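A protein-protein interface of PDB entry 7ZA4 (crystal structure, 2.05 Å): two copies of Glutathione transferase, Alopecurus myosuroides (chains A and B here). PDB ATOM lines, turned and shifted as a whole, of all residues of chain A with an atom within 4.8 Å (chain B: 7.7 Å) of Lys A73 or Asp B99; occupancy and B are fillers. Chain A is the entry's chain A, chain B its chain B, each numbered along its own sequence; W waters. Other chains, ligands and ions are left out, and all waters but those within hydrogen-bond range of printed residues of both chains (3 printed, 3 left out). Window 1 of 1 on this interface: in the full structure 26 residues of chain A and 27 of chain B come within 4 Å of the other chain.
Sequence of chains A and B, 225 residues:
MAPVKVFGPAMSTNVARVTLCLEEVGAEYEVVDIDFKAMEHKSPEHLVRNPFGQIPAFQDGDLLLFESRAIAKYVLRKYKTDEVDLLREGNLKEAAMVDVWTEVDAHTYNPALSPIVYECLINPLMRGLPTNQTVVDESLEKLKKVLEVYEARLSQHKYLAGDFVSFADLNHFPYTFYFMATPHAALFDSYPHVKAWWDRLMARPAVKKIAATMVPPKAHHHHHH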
ATOM      1  N   ARG A  69     -16.816  12.787 -24.151  1.00  0.00           N
ATOM      2  CA  ARG A  69     -17.554  11.538 -24.376  1.00  0.00           C
ATOM      3  C   ARG A  69     -18.718  11.387 -23.395  1.00  0.00           C
ATOM      4  O   ARG A  69     -19.812  10.946 -23.775  1.00  0.00           O
ATOM      5  CB  ARG A  69     -16.614  10.326 -24.268  1.00  0.00           C
ATOM      6  CG  ARG A  69     -15.663  10.162 -25.453  1.00  0.00           C
ATOM      7  CD  ARG A  69     -15.076   8.730 -25.573  1.00  0.00           C
ATOM      8  NE  ARG A  69     -14.227   8.617 -26.752  1.00  0.00           N
ATOM      9  CZ  ARG A  69     -13.011   9.135 -26.838  1.00  0.00           C
ATOM     10  NH1 ARG A  69     -12.440   9.717 -25.800  1.00  0.00           N
ATOM     11  NH2 ARG A  69     -12.359   9.088 -28.004  1.00  0.00           N
ATOM     12  N   ALA A  70     -18.504  11.717 -22.122  1.00  0.00           N
ATOM     13  CA  ALA A  70     -19.605  11.664 -21.166  1.00  0.00           C
ATOM     14  C   ALA A  70     -20.697  12.650 -21.540  1.00  0.00           C
ATOM     15  O   ALA A  70     -21.889  12.323 -21.477  1.00  0.00           O
ATOM     16  CB  ALA A  70     -19.096  11.947 -19.739  1.00  0.00           C
ATOM     17  N   ILE A  71     -20.311  13.862 -21.946  1.00  0.00           N
ATOM     18  CA  ILE A  71     -21.293  14.863 -22.360  1.00  0.00           C
ATOM     19  C   ILE A  71     -22.045  14.388 -23.599  1.00  0.00           C
ATOM     20  O   ILE A  71     -23.282  14.476 -23.675  1.00  0.00           O
ATOM     21  CB  ILE A  71     -20.610  16.216 -22.617  1.00  0.00           C
ATOM     22  CG1 ILE A  71     -20.076  16.843 -21.323  1.00  0.00           C
ATOM     23  CG2 ILE A  71     -21.588  17.185 -23.285  1.00  0.00           C
ATOM     24  CD1 ILE A  71     -18.946  17.815 -21.596  1.00  0.00           C
ATOM     25  N   ALA A  72     -21.303  13.898 -24.602  1.00  0.00           N
ATOM     26  CA  ALA A  72     -21.942  13.435 -25.833  1.00  0.00           C
ATOM     27  C   ALA A  72     -23.016  12.406 -25.521  1.00  0.00           C
ATOM     28  O   ALA A  72     -24.144  12.497 -26.028  1.00  0.00           O
ATOM     29  CB  ALA A  72     -20.899  12.866 -26.798  1.00  0.00           C
ATOM     30  N   LYS A  73     -22.697  11.444 -24.648  1.00  0.00           N
ATOM     31  CA  LYS A  73     -23.676  10.432 -24.276  1.00  0.00           C
ATOM     32  C   LYS A  73     -24.839  11.017 -23.489  1.00  0.00           C
ATOM     33  O   LYS A  73     -25.992  10.601 -23.679  1.00  0.00           O
ATOM     34  CB  LYS A  73     -23.004   9.321 -23.486  1.00  0.00           C
ATOM     35  CG  LYS A  73     -22.383   8.227 -24.378  1.00  0.00           C
ATOM     36  CD  LYS A  73     -22.111   6.980 -23.544  1.00  0.00           C
ATOM     37  CE  LYS A  73     -20.829   7.114 -22.740  1.00  0.00           C
ATOM     38  NZ  LYS A  73     -20.612   5.890 -21.924  1.00  0.00           N
ATOM     39  N   TYR A  74     -24.565  11.966 -22.584  1.00  0.00           N
ATOM     40  CA  TYR A  74     -25.656  12.640 -21.895  1.00  0.00           C
ATOM     41  C   TYR A  74     -26.629  13.221 -22.908  1.00  0.00           C
ATOM     42  O   TYR A  74     -27.845  13.021 -22.810  1.00  0.00           O
ATOM     43  CB  TYR A  74     -25.101  13.730 -20.963  1.00  0.00           C
ATOM     44  CG  TYR A  74     -26.175  14.603 -20.350  1.00  0.00           C
ATOM     45  CD1 TYR A  74     -26.581  15.762 -20.983  1.00  0.00           C
ATOM     46  CD2 TYR A  74     -26.794  14.259 -19.144  1.00  0.00           C
ATOM     47  CE1 TYR A  74     -27.574  16.572 -20.443  1.00  0.00           C
ATOM     48  CE2 TYR A  74     -27.787  15.067 -18.592  1.00  0.00           C
ATOM     49  CZ  TYR A  74     -28.166  16.223 -19.258  1.00  0.00           C
ATOM     50  OH  TYR A  74     -29.141  17.050 -18.771  1.00  0.00           O
ATOM     51  N   VAL A  75     -26.093  13.893 -23.931  1.00  0.00           N
ATOM     52  CA  VAL A  75     -26.914  14.553 -24.939  1.00  0.00           C
ATOM     53  C   VAL A  75     -27.695  13.537 -25.765  1.00  0.00           C
ATOM     54  O   VAL A  75     -28.886  13.734 -26.052  1.00  0.00           O
ATOM     55  CB  VAL A  75     -26.013  15.457 -25.807  1.00  0.00           C
ATOM     56  CG1 VAL A  75     -26.675  15.804 -27.106  1.00  0.00           C
ATOM     57  CG2 VAL A  75     -25.625  16.722 -25.020  1.00  0.00           C
ATOM     58  N   LEU A  76     -27.043  12.431 -26.164  1.00  0.00           N
ATOM     59  CA  LEU A  76     -27.750  11.379 -26.883  1.00  0.00           C
ATOM     60  C   LEU A  76     -28.840  10.757 -26.023  1.00  0.00           C
ATOM     61  O   LEU A  76     -29.892  10.364 -26.533  1.00  0.00           O
ATOM     62  CB  LEU A  76     -26.768  10.294 -27.353  1.00  0.00           C
ATOM     63  CG  LEU A  76     -25.716  10.823 -28.334  1.00  0.00           C
ATOM     64  CD1 LEU A  76     -24.730   9.738 -28.738  1.00  0.00           C
ATOM     65  CD2 LEU A  76     -26.407  11.393 -29.540  1.00  0.00           C
ATOM     66  N   ARG A  77     -28.601  10.628 -24.718  1.00  0.00           N
ATOM     67  CA  ARG A  77     -29.624  10.048 -23.852  1.00  0.00           C
ATOM     68  C   ARG A  77     -30.757  11.042 -23.613  1.00  0.00           C
ATOM     69  O   ARG A  77     -31.939  10.691 -23.698  1.00  0.00           O
ATOM     70  CB  ARG A  77     -29.008   9.625 -22.522  1.00  0.00           C
ATOM     71  CG  ARG A  77     -28.447   8.232 -22.483  1.00  0.00           C
ATOM     72  CD  ARG A  77     -27.808   7.954 -21.128  1.00  0.00           C
ATOM     73  NE  ARG A  77     -26.916   6.802 -21.209  1.00  0.00           N
ATOM     74  CZ  ARG A  77     -25.673   6.788 -20.750  1.00  0.00           C
ATOM     75  NH1 ARG A  77     -25.149   7.843 -20.132  1.00  0.00           N
ATOM     76  NH2 ARG A  77     -24.937   5.692 -20.913  1.00  0.00           N
ATOM     77  N   LYS A  78     -30.409  12.292 -23.303  1.00  0.00           N
ATOM     78  CA  LYS A  78     -31.430  13.270 -22.945  1.00  0.00           C
ATOM     79  C   LYS A  78     -32.441  13.447 -24.071  1.00  0.00           C
ATOM     80  O   LYS A  78     -33.650  13.383 -23.844  1.00  0.00           O
ATOM     81  CB  LYS A  78     -30.782  14.604 -22.589  1.00  0.00           C
ATOM     82  CG  LYS A  78     -31.700  15.537 -21.783  1.00  0.00           C
ATOM     83  CD  LYS A  78     -31.625  16.953 -22.319  1.00  0.00           C
ATOM     84  CE  LYS A  78     -32.133  18.007 -21.330  1.00  0.00           C
ATOM     85  NZ  LYS A  78     -31.708  19.355 -21.814  1.00  0.00           N
ATOM     86  N   LEU A  87     -27.554   5.523 -29.330  1.00  0.00           N
ATOM     87  CA  LEU A  87     -26.886   4.646 -28.377  1.00  0.00           C
ATOM     88  C   LEU A  87     -27.491   3.252 -28.306  1.00  0.00           C
ATOM     89  O   LEU A  87     -26.790   2.308 -27.924  1.00  0.00           O
ATOM     90  CB  LEU A  87     -26.908   5.265 -26.967  1.00  0.00           C
ATOM     91  CG  LEU A  87     -26.057   6.520 -26.781  1.00  0.00           C
ATOM     92  CD1 LEU A  87     -26.240   7.157 -25.378  1.00  0.00           C
ATOM     93  CD2 LEU A  87     -24.592   6.209 -27.036  1.00  0.00           C
ATOM     94  N   PHE A 167     -23.508   6.429 -32.232  1.00  0.00           N
ATOM     95  CA  PHE A 167     -22.450   7.142 -31.520  1.00  0.00           C
ATOM     96  C   PHE A 167     -21.075   6.676 -31.992  1.00  0.00           C
ATOM     97  O   PHE A 167     -20.170   7.496 -32.197  1.00  0.00           O
ATOM     98  CB  PHE A 167     -22.648   6.929 -30.016  1.00  0.00           C
ATOM     99  CG  PHE A 167     -21.719   7.734 -29.124  1.00  0.00           C
ATOM    100  CD1 PHE A 167     -21.440   9.063 -29.389  1.00  0.00           C
ATOM    101  CD2 PHE A 167     -21.200   7.167 -27.966  1.00  0.00           C
ATOM    102  CE1 PHE A 167     -20.616   9.819 -28.522  1.00  0.00           C
ATOM    103  CE2 PHE A 167     -20.371   7.890 -27.116  1.00  0.00           C
ATOM    104  CZ  PHE A 167     -20.091   9.235 -27.384  1.00  0.00           C
ATOM    105  N   LYS B  73     -20.327  -3.706 -19.812  1.00  0.00           N
ATOM    106  CA  LYS B  73     -21.561  -2.930 -19.900  1.00  0.00           C
ATOM    107  C   LYS B  73     -22.727  -3.788 -20.368  1.00  0.00           C
ATOM    108  O   LYS B  73     -23.858  -3.604 -19.906  1.00  0.00           O
ATOM    109  CB  LYS B  73     -21.359  -1.743 -20.823  1.00  0.00           C
ATOM    110  CG  LYS B  73     -20.852  -0.495 -20.104  1.00  0.00           C
ATOM    111  CD  LYS B  73     -20.940   0.724 -21.010  1.00  0.00           C
ATOM    112  CE  LYS B  73     -19.747   0.764 -21.965  1.00  0.00           C
ATOM    113  NZ  LYS B  73     -19.852   1.919 -22.880  1.00  0.00           N
ATOM    114  N   ARG B  77     -25.954  -4.373 -18.085  1.00  0.00           N
ATOM    115  CA  ARG B  77     -27.246  -4.011 -18.657  1.00  0.00           C
ATOM    116  C   ARG B  77     -28.231  -5.169 -18.576  1.00  0.00           C
ATOM    117  O   ARG B  77     -29.378  -4.988 -18.157  1.00  0.00           O
ATOM    118  CB  ARG B  77     -27.078  -3.559 -20.106  1.00  0.00           C
ATOM    119  CG  ARG B  77     -26.748  -2.077 -20.245  1.00  0.00           C
ATOM    120  CD  ARG B  77     -26.764  -1.603 -21.690  1.00  0.00           C
ATOM    121  NE  ARG B  77     -26.112  -0.303 -21.801  1.00  0.00           N
ATOM    122  CZ  ARG B  77     -25.085  -0.059 -22.601  1.00  0.00           C
ATOM    123  NH1 ARG B  77     -24.604  -0.994 -23.410  1.00  0.00           N
ATOM    124  NH2 ARG B  77     -24.526   1.146 -22.589  1.00  0.00           N
ATOM    125  N   LEU B  87     -24.898   0.986 -13.736  1.00  0.00           N
ATOM    126  CA  LEU B  87     -24.697   2.008 -14.758  1.00  0.00           C
ATOM    127  C   LEU B  87     -25.593   3.230 -14.606  1.00  0.00           C
ATOM    128  O   LEU B  87     -25.247   4.284 -15.147  1.00  0.00           O
ATOM    129  CB  LEU B  87     -24.919   1.430 -16.165  1.00  0.00           C
ATOM    130  CG  LEU B  87     -23.949   0.330 -16.606  1.00  0.00           C
ATOM    131  CD1 LEU B  87     -24.532  -0.459 -17.762  1.00  0.00           C
ATOM    132  CD2 LEU B  87     -22.604   0.941 -16.995  1.00  0.00           C
ATOM    133  N   GLU B  89     -28.428   4.164 -15.938  1.00  0.00           N
ATOM    134  CA  GLU B  89     -28.791   4.765 -17.225  1.00  0.00           C
ATOM    135  C   GLU B  89     -30.181   5.402 -17.212  1.00  0.00           C
ATOM    136  O   GLU B  89     -30.479   6.222 -18.090  1.00  0.00           O
ATOM    137  CB  GLU B  89     -28.689   3.720 -18.354  1.00  0.00           C
ATOM    138  CG  GLU B  89     -27.253   3.523 -18.850  1.00  0.00           C
ATOM    139  CD  GLU B  89     -27.075   2.341 -19.815  1.00  0.00           C
ATOM    140  OE1 GLU B  89     -28.046   1.587 -20.056  1.00  0.00           O
ATOM    141  OE2 GLU B  89     -25.948   2.169 -20.333  1.00  0.00           O
ATOM    142  N   LEU B  92     -30.105  10.419 -15.831  1.00  0.00           N
ATOM    143  CA  LEU B  92     -29.145  11.083 -16.711  1.00  0.00           C
ATOM    144  C   LEU B  92     -27.952  11.637 -15.945  1.00  0.00           C
ATOM    145  O   LEU B  92     -26.804  11.507 -16.393  1.00  0.00           O
ATOM    146  CB  LEU B  92     -29.823  12.220 -17.472  1.00  0.00           C
ATOM    147  CG  LEU B  92     -30.912  11.930 -18.495  1.00  0.00           C
ATOM    148  CD1 LEU B  92     -31.057  13.176 -19.308  1.00  0.00           C
ATOM    149  CD2 LEU B  92     -30.599  10.712 -19.403  1.00  0.00           C
ATOM    150  N   LYS B  93     -28.202  12.280 -14.800  1.00  0.00           N
ATOM    151  CA  LYS B  93     -27.114  12.911 -14.065  1.00  0.00           C
ATOM    152  C   LYS B  93     -26.188  11.873 -13.443  1.00  0.00           C
ATOM    153  O   LYS B  93     -24.962  11.995 -13.536  1.00  0.00           O
ATOM    154  CB  LYS B  93     -27.674  13.863 -12.994  1.00  0.00           C
ATOM    155  CG  LYS B  93     -28.330  15.125 -13.580  1.00  0.00           C
ATOM    156  CD  LYS B  93     -28.517  16.227 -12.514  1.00  0.00           C
ATOM    157  CE  LYS B  93     -29.150  17.491 -13.107  1.00  0.00           C
ATOM    158  NZ  LYS B  93     -29.195  18.637 -12.130  1.00  0.00           N
ATOM    159  N   GLU B  94     -26.752  10.870 -12.764  1.00  0.00           N
ATOM    160  CA  GLU B  94     -25.917   9.814 -12.198  1.00  0.00           C
ATOM    161  C   GLU B  94     -25.145   9.076 -13.296  1.00  0.00           C
ATOM    162  O   GLU B  94     -23.949   8.800 -13.154  1.00  0.00           O
ATOM    163  CB  GLU B  94     -26.782   8.832 -11.407  1.00  0.00           C
ATOM    164  CG  GLU B  94     -27.387   9.403 -10.128  1.00  0.00           C
ATOM    165  CD  GLU B  94     -28.355   8.431  -9.469  1.00  0.00           C
ATOM    166  OE1 GLU B  94     -28.735   7.437 -10.125  1.00  0.00           O
ATOM    167  OE2 GLU B  94     -28.721   8.650  -8.291  1.00  0.00           O
ATOM    168  N   ALA B  95     -25.812   8.762 -14.405  1.00  0.00           N
ATOM    169  CA  ALA B  95     -25.139   8.062 -15.499  1.00  0.00           C
ATOM    170  C   ALA B  95     -23.992   8.886 -16.067  1.00  0.00           C
ATOM    171  O   ALA B  95     -22.995   8.325 -16.538  1.00  0.00           O
ATOM    172  CB  ALA B  95     -26.140   7.730 -16.603  1.00  0.00           C
ATOM    173  N   ALA B  96     -24.110  10.220 -16.031  1.00  0.00           N
ATOM    174  CA  ALA B  96     -23.022  11.036 -16.551  1.00  0.00           C
ATOM    175  C   ALA B  96     -21.816  10.972 -15.630  1.00  0.00           C
ATOM    176  O   ALA B  96     -20.670  11.004 -16.094  1.00  0.00           O
ATOM    177  CB  ALA B  96     -23.484  12.481 -16.758  1.00  0.00           C
ATOM    178  N   MET B  97     -22.051  10.878 -14.317  1.00  0.00           N
ATOM    179  CA  MET B  97     -20.939  10.725 -13.386  1.00  0.00           C
ATOM    180  C   MET B  97     -20.291   9.347 -13.524  1.00  0.00           C
ATOM    181  O   MET B  97     -19.062   9.222 -13.490  1.00  0.00           O
ATOM    182  CB  MET B  97     -21.419  10.979 -11.960  1.00  0.00           C
ATOM    183  CG  MET B  97     -21.915  12.423 -11.729  1.00  0.00           C
ATOM    184  SD  MET B  97     -20.559  13.574 -12.025  1.00  0.00           S
ATOM    185  CE  MET B  97     -21.003  14.283 -13.584  1.00  0.00           C
ATOM    186  N   VAL B  98     -21.092   8.302 -13.682  1.00  0.00           N
ATOM    187  CA  VAL B  98     -20.524   6.995 -14.018  1.00  0.00           C
ATOM    188  C   VAL B  98     -19.656   7.105 -15.269  1.00  0.00           C
ATOM    189  O   VAL B  98     -18.506   6.641 -15.300  1.00  0.00           O
ATOM    190  CB  VAL B  98     -21.644   5.958 -14.196  1.00  0.00           C
ATOM    191  CG1 VAL B  98     -21.060   4.571 -14.572  1.00  0.00           C
ATOM    192  CG2 VAL B  98     -22.503   5.898 -12.928  1.00  0.00           C
ATOM    193  N   ASP B  99     -20.187   7.767 -16.296  1.00  0.00           N
ATOM    194  CA  ASP B  99     -19.500   7.905 -17.576  1.00  0.00           C
ATOM    195  C   ASP B  99     -18.192   8.685 -17.454  1.00  0.00           C
ATOM    196  O   ASP B  99     -17.169   8.286 -18.029  1.00  0.00           O
ATOM    197  CB  ASP B  99     -20.439   8.578 -18.578  1.00  0.00           C
ATOM    198  CG  ASP B  99     -21.436   7.600 -19.193  1.00  0.00           C
ATOM    199  OD1 ASP B  99     -21.419   6.414 -18.785  1.00  0.00           O
ATOM    200  OD2 ASP B  99     -22.258   8.018 -20.049  1.00  0.00           O
ATOM    201  N   VAL B 100     -18.199   9.826 -16.745  1.00  0.00           N
ATOM    202  CA  VAL B 100     -16.975  10.619 -16.696  1.00  0.00           C
ATOM    203  C   VAL B 100     -15.873   9.835 -16.001  1.00  0.00           C
ATOM    204  O   VAL B 100     -14.714   9.856 -16.432  1.00  0.00           O
ATOM    205  CB  VAL B 100     -17.195  11.998 -16.021  1.00  0.00           C
ATOM    206  CG1 VAL B 100     -17.753  11.859 -14.646  1.00  0.00           C
ATOM    207  CG2 VAL B 100     -15.882  12.701 -15.890  1.00  0.00           C
ATOM    208  N   TRP B 101     -16.203   9.117 -14.924  1.00  0.00           N
ATOM    209  CA  TRP B 101     -15.135   8.491 -14.155  1.00  0.00           C
ATOM    210  C   TRP B 101     -14.675   7.176 -14.771  1.00  0.00           C
ATOM    211  O   TRP B 101     -13.518   6.779 -14.565  1.00  0.00           O
ATOM    212  CB  TRP B 101     -15.572   8.321 -12.683  1.00  0.00           C
ATOM    213  CG  TRP B 101     -15.506   9.684 -11.998  1.00  0.00           C
ATOM    214  CD1 TRP B 101     -16.524  10.596 -11.856  1.00  0.00           C
ATOM    215  CD2 TRP B 101     -14.334  10.308 -11.480  1.00  0.00           C
ATOM    216  NE1 TRP B 101     -16.056  11.739 -11.239  1.00  0.00           N
ATOM    217  CE2 TRP B 101     -14.713  11.583 -10.999  1.00  0.00           C
ATOM    218  CE3 TRP B 101     -12.995   9.899 -11.345  1.00  0.00           C
ATOM    219  CZ2 TRP B 101     -13.805  12.447 -10.406  1.00  0.00           C
ATOM    220  CZ3 TRP B 101     -12.092  10.766 -10.764  1.00  0.00           C
ATOM    221  CH2 TRP B 101     -12.504  12.023 -10.293  1.00  0.00           C
ATOM    222  N   THR B 102     -15.533   6.523 -15.548  1.00  0.00           N
ATOM    223  CA  THR B 102     -15.062   5.454 -16.435  1.00  0.00           C
ATOM    224  C   THR B 102     -14.076   5.996 -17.466  1.00  0.00           C
ATOM    225  O   THR B 102     -13.062   5.351 -17.756  1.00  0.00           O
ATOM    226  CB  THR B 102     -16.266   4.778 -17.095  1.00  0.00           C
ATOM    227  OG1 THR B 102     -17.072   4.194 -16.064  1.00  0.00           O
ATOM    228  CG2 THR B 102     -15.855   3.659 -18.090  1.00  0.00           C
ATOM    229  N   GLU B 103     -14.316   7.209 -17.990  1.00  0.00           N
ATOM    230  CA  GLU B 103     -13.358   7.795 -18.931  1.00  0.00           C
ATOM    231  C   GLU B 103     -12.058   8.185 -18.241  1.00  0.00           C
ATOM    232  O   GLU B 103     -10.981   8.047 -18.826  1.00  0.00           O
ATOM    233  CB  GLU B 103     -13.954   9.015 -19.638  1.00  0.00           C
ATOM    234  CG  GLU B 103     -15.181   8.745 -20.515  1.00  0.00           C
ATOM    235  CD  GLU B 103     -14.920   7.714 -21.612  1.00  0.00           C
ATOM    236  OE1 GLU B 103     -13.856   7.810 -22.300  1.00  0.00           O
ATOM    237  OE2 GLU B 103     -15.793   6.825 -21.782  1.00  0.00           O
ATOM    238  N   VAL B 104     -12.130   8.721 -17.012  1.00  0.00           N
ATOM    239  CA  VAL B 104     -10.900   9.057 -16.297  1.00  0.00           C
ATOM    240  C   VAL B 104     -10.038   7.812 -16.117  1.00  0.00           C
ATOM    241  O   VAL B 104      -8.811   7.845 -16.308  1.00  0.00           O
ATOM    242  CB  VAL B 104     -11.221   9.709 -14.939  1.00  0.00           C
ATOM    243  CG1 VAL B 104      -9.945   9.877 -14.149  1.00  0.00           C
ATOM    244  CG2 VAL B 104     -11.960  11.028 -15.148  1.00  0.00           C
ATOM    245  N   ASP B 105     -10.658   6.708 -15.690  1.00  0.00           N
ATOM    246  CA  ASP B 105      -9.933   5.438 -15.649  1.00  0.00           C
ATOM    247  C   ASP B 105      -9.236   5.178 -16.973  1.00  0.00           C
ATOM    248  O   ASP B 105      -8.001   5.101 -17.041  1.00  0.00           O
ATOM    249  CB  ASP B 105     -10.859   4.268 -15.328  1.00  0.00           C
ATOM    250  CG  ASP B 105     -10.126   2.920 -15.416  1.00  0.00           C
ATOM    251  OD1 ASP B 105      -9.120   2.745 -14.695  1.00  0.00           O
ATOM    252  OD2 ASP B 105     -10.530   2.034 -16.208  1.00  0.00           O
ATOM    253  N   ALA B 161     -18.591   7.986  -8.613  1.00  0.00           N
ATOM    254  CA  ALA B 161     -19.752   8.605  -9.243  1.00  0.00           C
ATOM    255  C   ALA B 161     -20.659   9.292  -8.241  1.00  0.00           C
ATOM    256  O   ALA B 161     -21.615   9.960  -8.648  1.00  0.00           O
ATOM    257  CB  ALA B 161     -20.574   7.580 -10.023  1.00  0.00           C
ATOM    258  N   SER B 166     -20.424   2.039  -8.597  1.00  0.00           N
ATOM    259  CA  SER B 166     -20.830   1.997  -9.993  1.00  0.00           C
ATOM    260  C   SER B 166     -19.763   1.327 -10.848  1.00  0.00           C
ATOM    261  O   SER B 166     -18.650   1.039 -10.391  1.00  0.00           O
ATOM    262  CB  SER B 166     -21.097   3.397 -10.524  1.00  0.00           C
ATOM    263  OG  SER B 166     -19.862   4.063 -10.729  1.00  0.00           O
ATOM    264  N   PHE B 167     -20.119   1.123 -12.125  1.00  0.00           N
ATOM    265  CA  PHE B 167     -19.159   0.676 -13.135  1.00  0.00           C
ATOM    266  C   PHE B 167     -17.857   1.450 -13.036  1.00  0.00           C
ATOM    267  O   PHE B 167     -16.776   0.890 -13.250  1.00  0.00           O
ATOM    268  CB  PHE B 167     -19.767   0.834 -14.535  1.00  0.00           C
ATOM    269  CG  PHE B 167     -18.957   0.191 -15.663  1.00  0.00           C
ATOM    270  CD1 PHE B 167     -18.377  -1.057 -15.508  1.00  0.00           C
ATOM    271  CD2 PHE B 167     -18.816   0.842 -16.892  1.00  0.00           C
ATOM    272  CE1 PHE B 167     -17.664  -1.666 -16.576  1.00  0.00           C
ATOM    273  CE2 PHE B 167     -18.098   0.264 -17.940  1.00  0.00           C
ATOM    274  CZ  PHE B 167     -17.534  -1.007 -17.794  1.00  0.00           C
ATOM    275  N   ALA B 168     -17.936   2.742 -12.690  1.00  0.00           N
ATOM    276  CA  ALA B 168     -16.724   3.537 -12.637  1.00  0.00           C
ATOM    277  C   ALA B 168     -15.759   2.987 -11.604  1.00  0.00           C
ATOM    278  O   ALA B 168     -14.554   2.889 -11.862  1.00  0.00           O
ATOM    279  CB  ALA B 168     -17.060   5.001 -12.347  1.00  0.00           C
ATOM    280  N   ASN B 171     -14.221  -0.522 -12.700  1.00  0.00           N
ATOM    281  CA  ASN B 171     -13.180  -0.464 -13.726  1.00  0.00           C
ATOM    282  C   ASN B 171     -11.789  -0.320 -13.142  1.00  0.00           C
ATOM    283  O   ASN B 171     -10.817  -0.763 -13.764  1.00  0.00           O
ATOM    284  CB  ASN B 171     -13.430   0.715 -14.672  1.00  0.00           C
ATOM    285  CG  ASN B 171     -14.365   0.364 -15.793  1.00  0.00           C
ATOM    286  OD1 ASN B 171     -14.132  -0.597 -16.525  1.00  0.00           O
ATOM    287  ND2 ASN B 171     -15.422   1.163 -15.959  1.00  0.00           N
HETATM  288  O   HOH W   1     -12.802  10.137 -23.182  1.00  0.00           O
HETATM  289  O   HOH W   2     -23.325  10.562 -19.824  1.00  0.00           O
HETATM  290  O   HOH W   3     -25.984  10.777 -19.279  1.00  0.00           O
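Water W1 bridges the guanidinium group (NH1) of Arg A69 and the side-chain carboxylate (OE1) of Glu B103.
Water W2 lies within hydrogen-bond range of the side-chain carboxylate (OD2) of Asp B99, the backbone carbonyl oxygen (O) of Ala A70, the guanidinium group (NH1) of Arg A77 and the backbone NH (N) of Tyr A74.
Water W3 lies within hydrogen-bond range of O of Leu B92 (3.1 Å) and NH1 of Arg A77 (3.2 Å).
Of chain B, only Asp B99 (3.2 Å) comes within 4 Å of Lys A73.
Of chain A, only Ala A70, Lys A73 and Arg A77 come within 4 Å of Asp B99.
No residue of chain B comes within 4 Å of Ala A72.
Of the printed residues of chain B, Ala A70 touches Asp B99 and Val B100.
Of the printed residues of chain A, Leu B92 touches Tyr A74 (3.7 Å), Arg A77 (3.7 Å) and Lys A78 (3.5 Å).
Of the printed residues of chain B, Tyr A74 touches Leu B92.
Thr B102 touches none of the printed residues of chain A.
Leu B87 touches none of the printed residues of chain A.
The nearest residue of chain B that does not touch Lys A73 is Lys B73 (4.2 Å).
The nearest printed residue of chain A that does not touch Asp B99 is Tyr A74 (5.2 Å).
Of the 12 printed residues of chain A, 6 touch a printed residue of chain B.
Hydrophobic or aromatic side chains of chain A within 4 Å of the printed part of chain B: Ala A70 and Tyr A74.
Of the 23 printed residues of chain B, 6 touch a printed residue of chain A.
Hydrophobic or aromatic side chains of chain B within 4 Å of the printed part of chain A: Leu B92 and Ala B95.
The guanidinium group (NH2) of Arg B77 lies within salt-bridge range of the side-chain carboxylate (OE2) of Glu B89 (2.9 Å).
NZ of Lys A73 lies within salt-bridge range of OD2 of Asp B99.
The guanidinium group of Arg A77 lies within salt-bridge range of the side-chain carboxylate of Glu B89 (3.7 Å).
The guanidinium group (NH1) of Arg A77 is in salt-bridge range of the side-chain carboxylate (OD2) of Asp B99 (2.9 Å).
4 positions are printed for both chains.
Of the 10 pairs that touch across the chains among the printed residues, none has its exchanged pair printed and touching as well.
Glu B103 touches Arg A69 (OE1 to CD, 3.6 Å).
CB of Ala A70 touches CB of Asp B99, at 3.8 Å.
CB of Ala A70 touches N of Val B100, at 3.8 Å.
Leu B92 touches Tyr A74 (CB to CE2, 3.7 Å).
Arg A77 touches Leu B92.
Ala B95 touches Arg A77 (CB to NH1, 3.7 Å).
Leu B92 touches Lys A78 (CD1 to CG, 3.5 Å).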
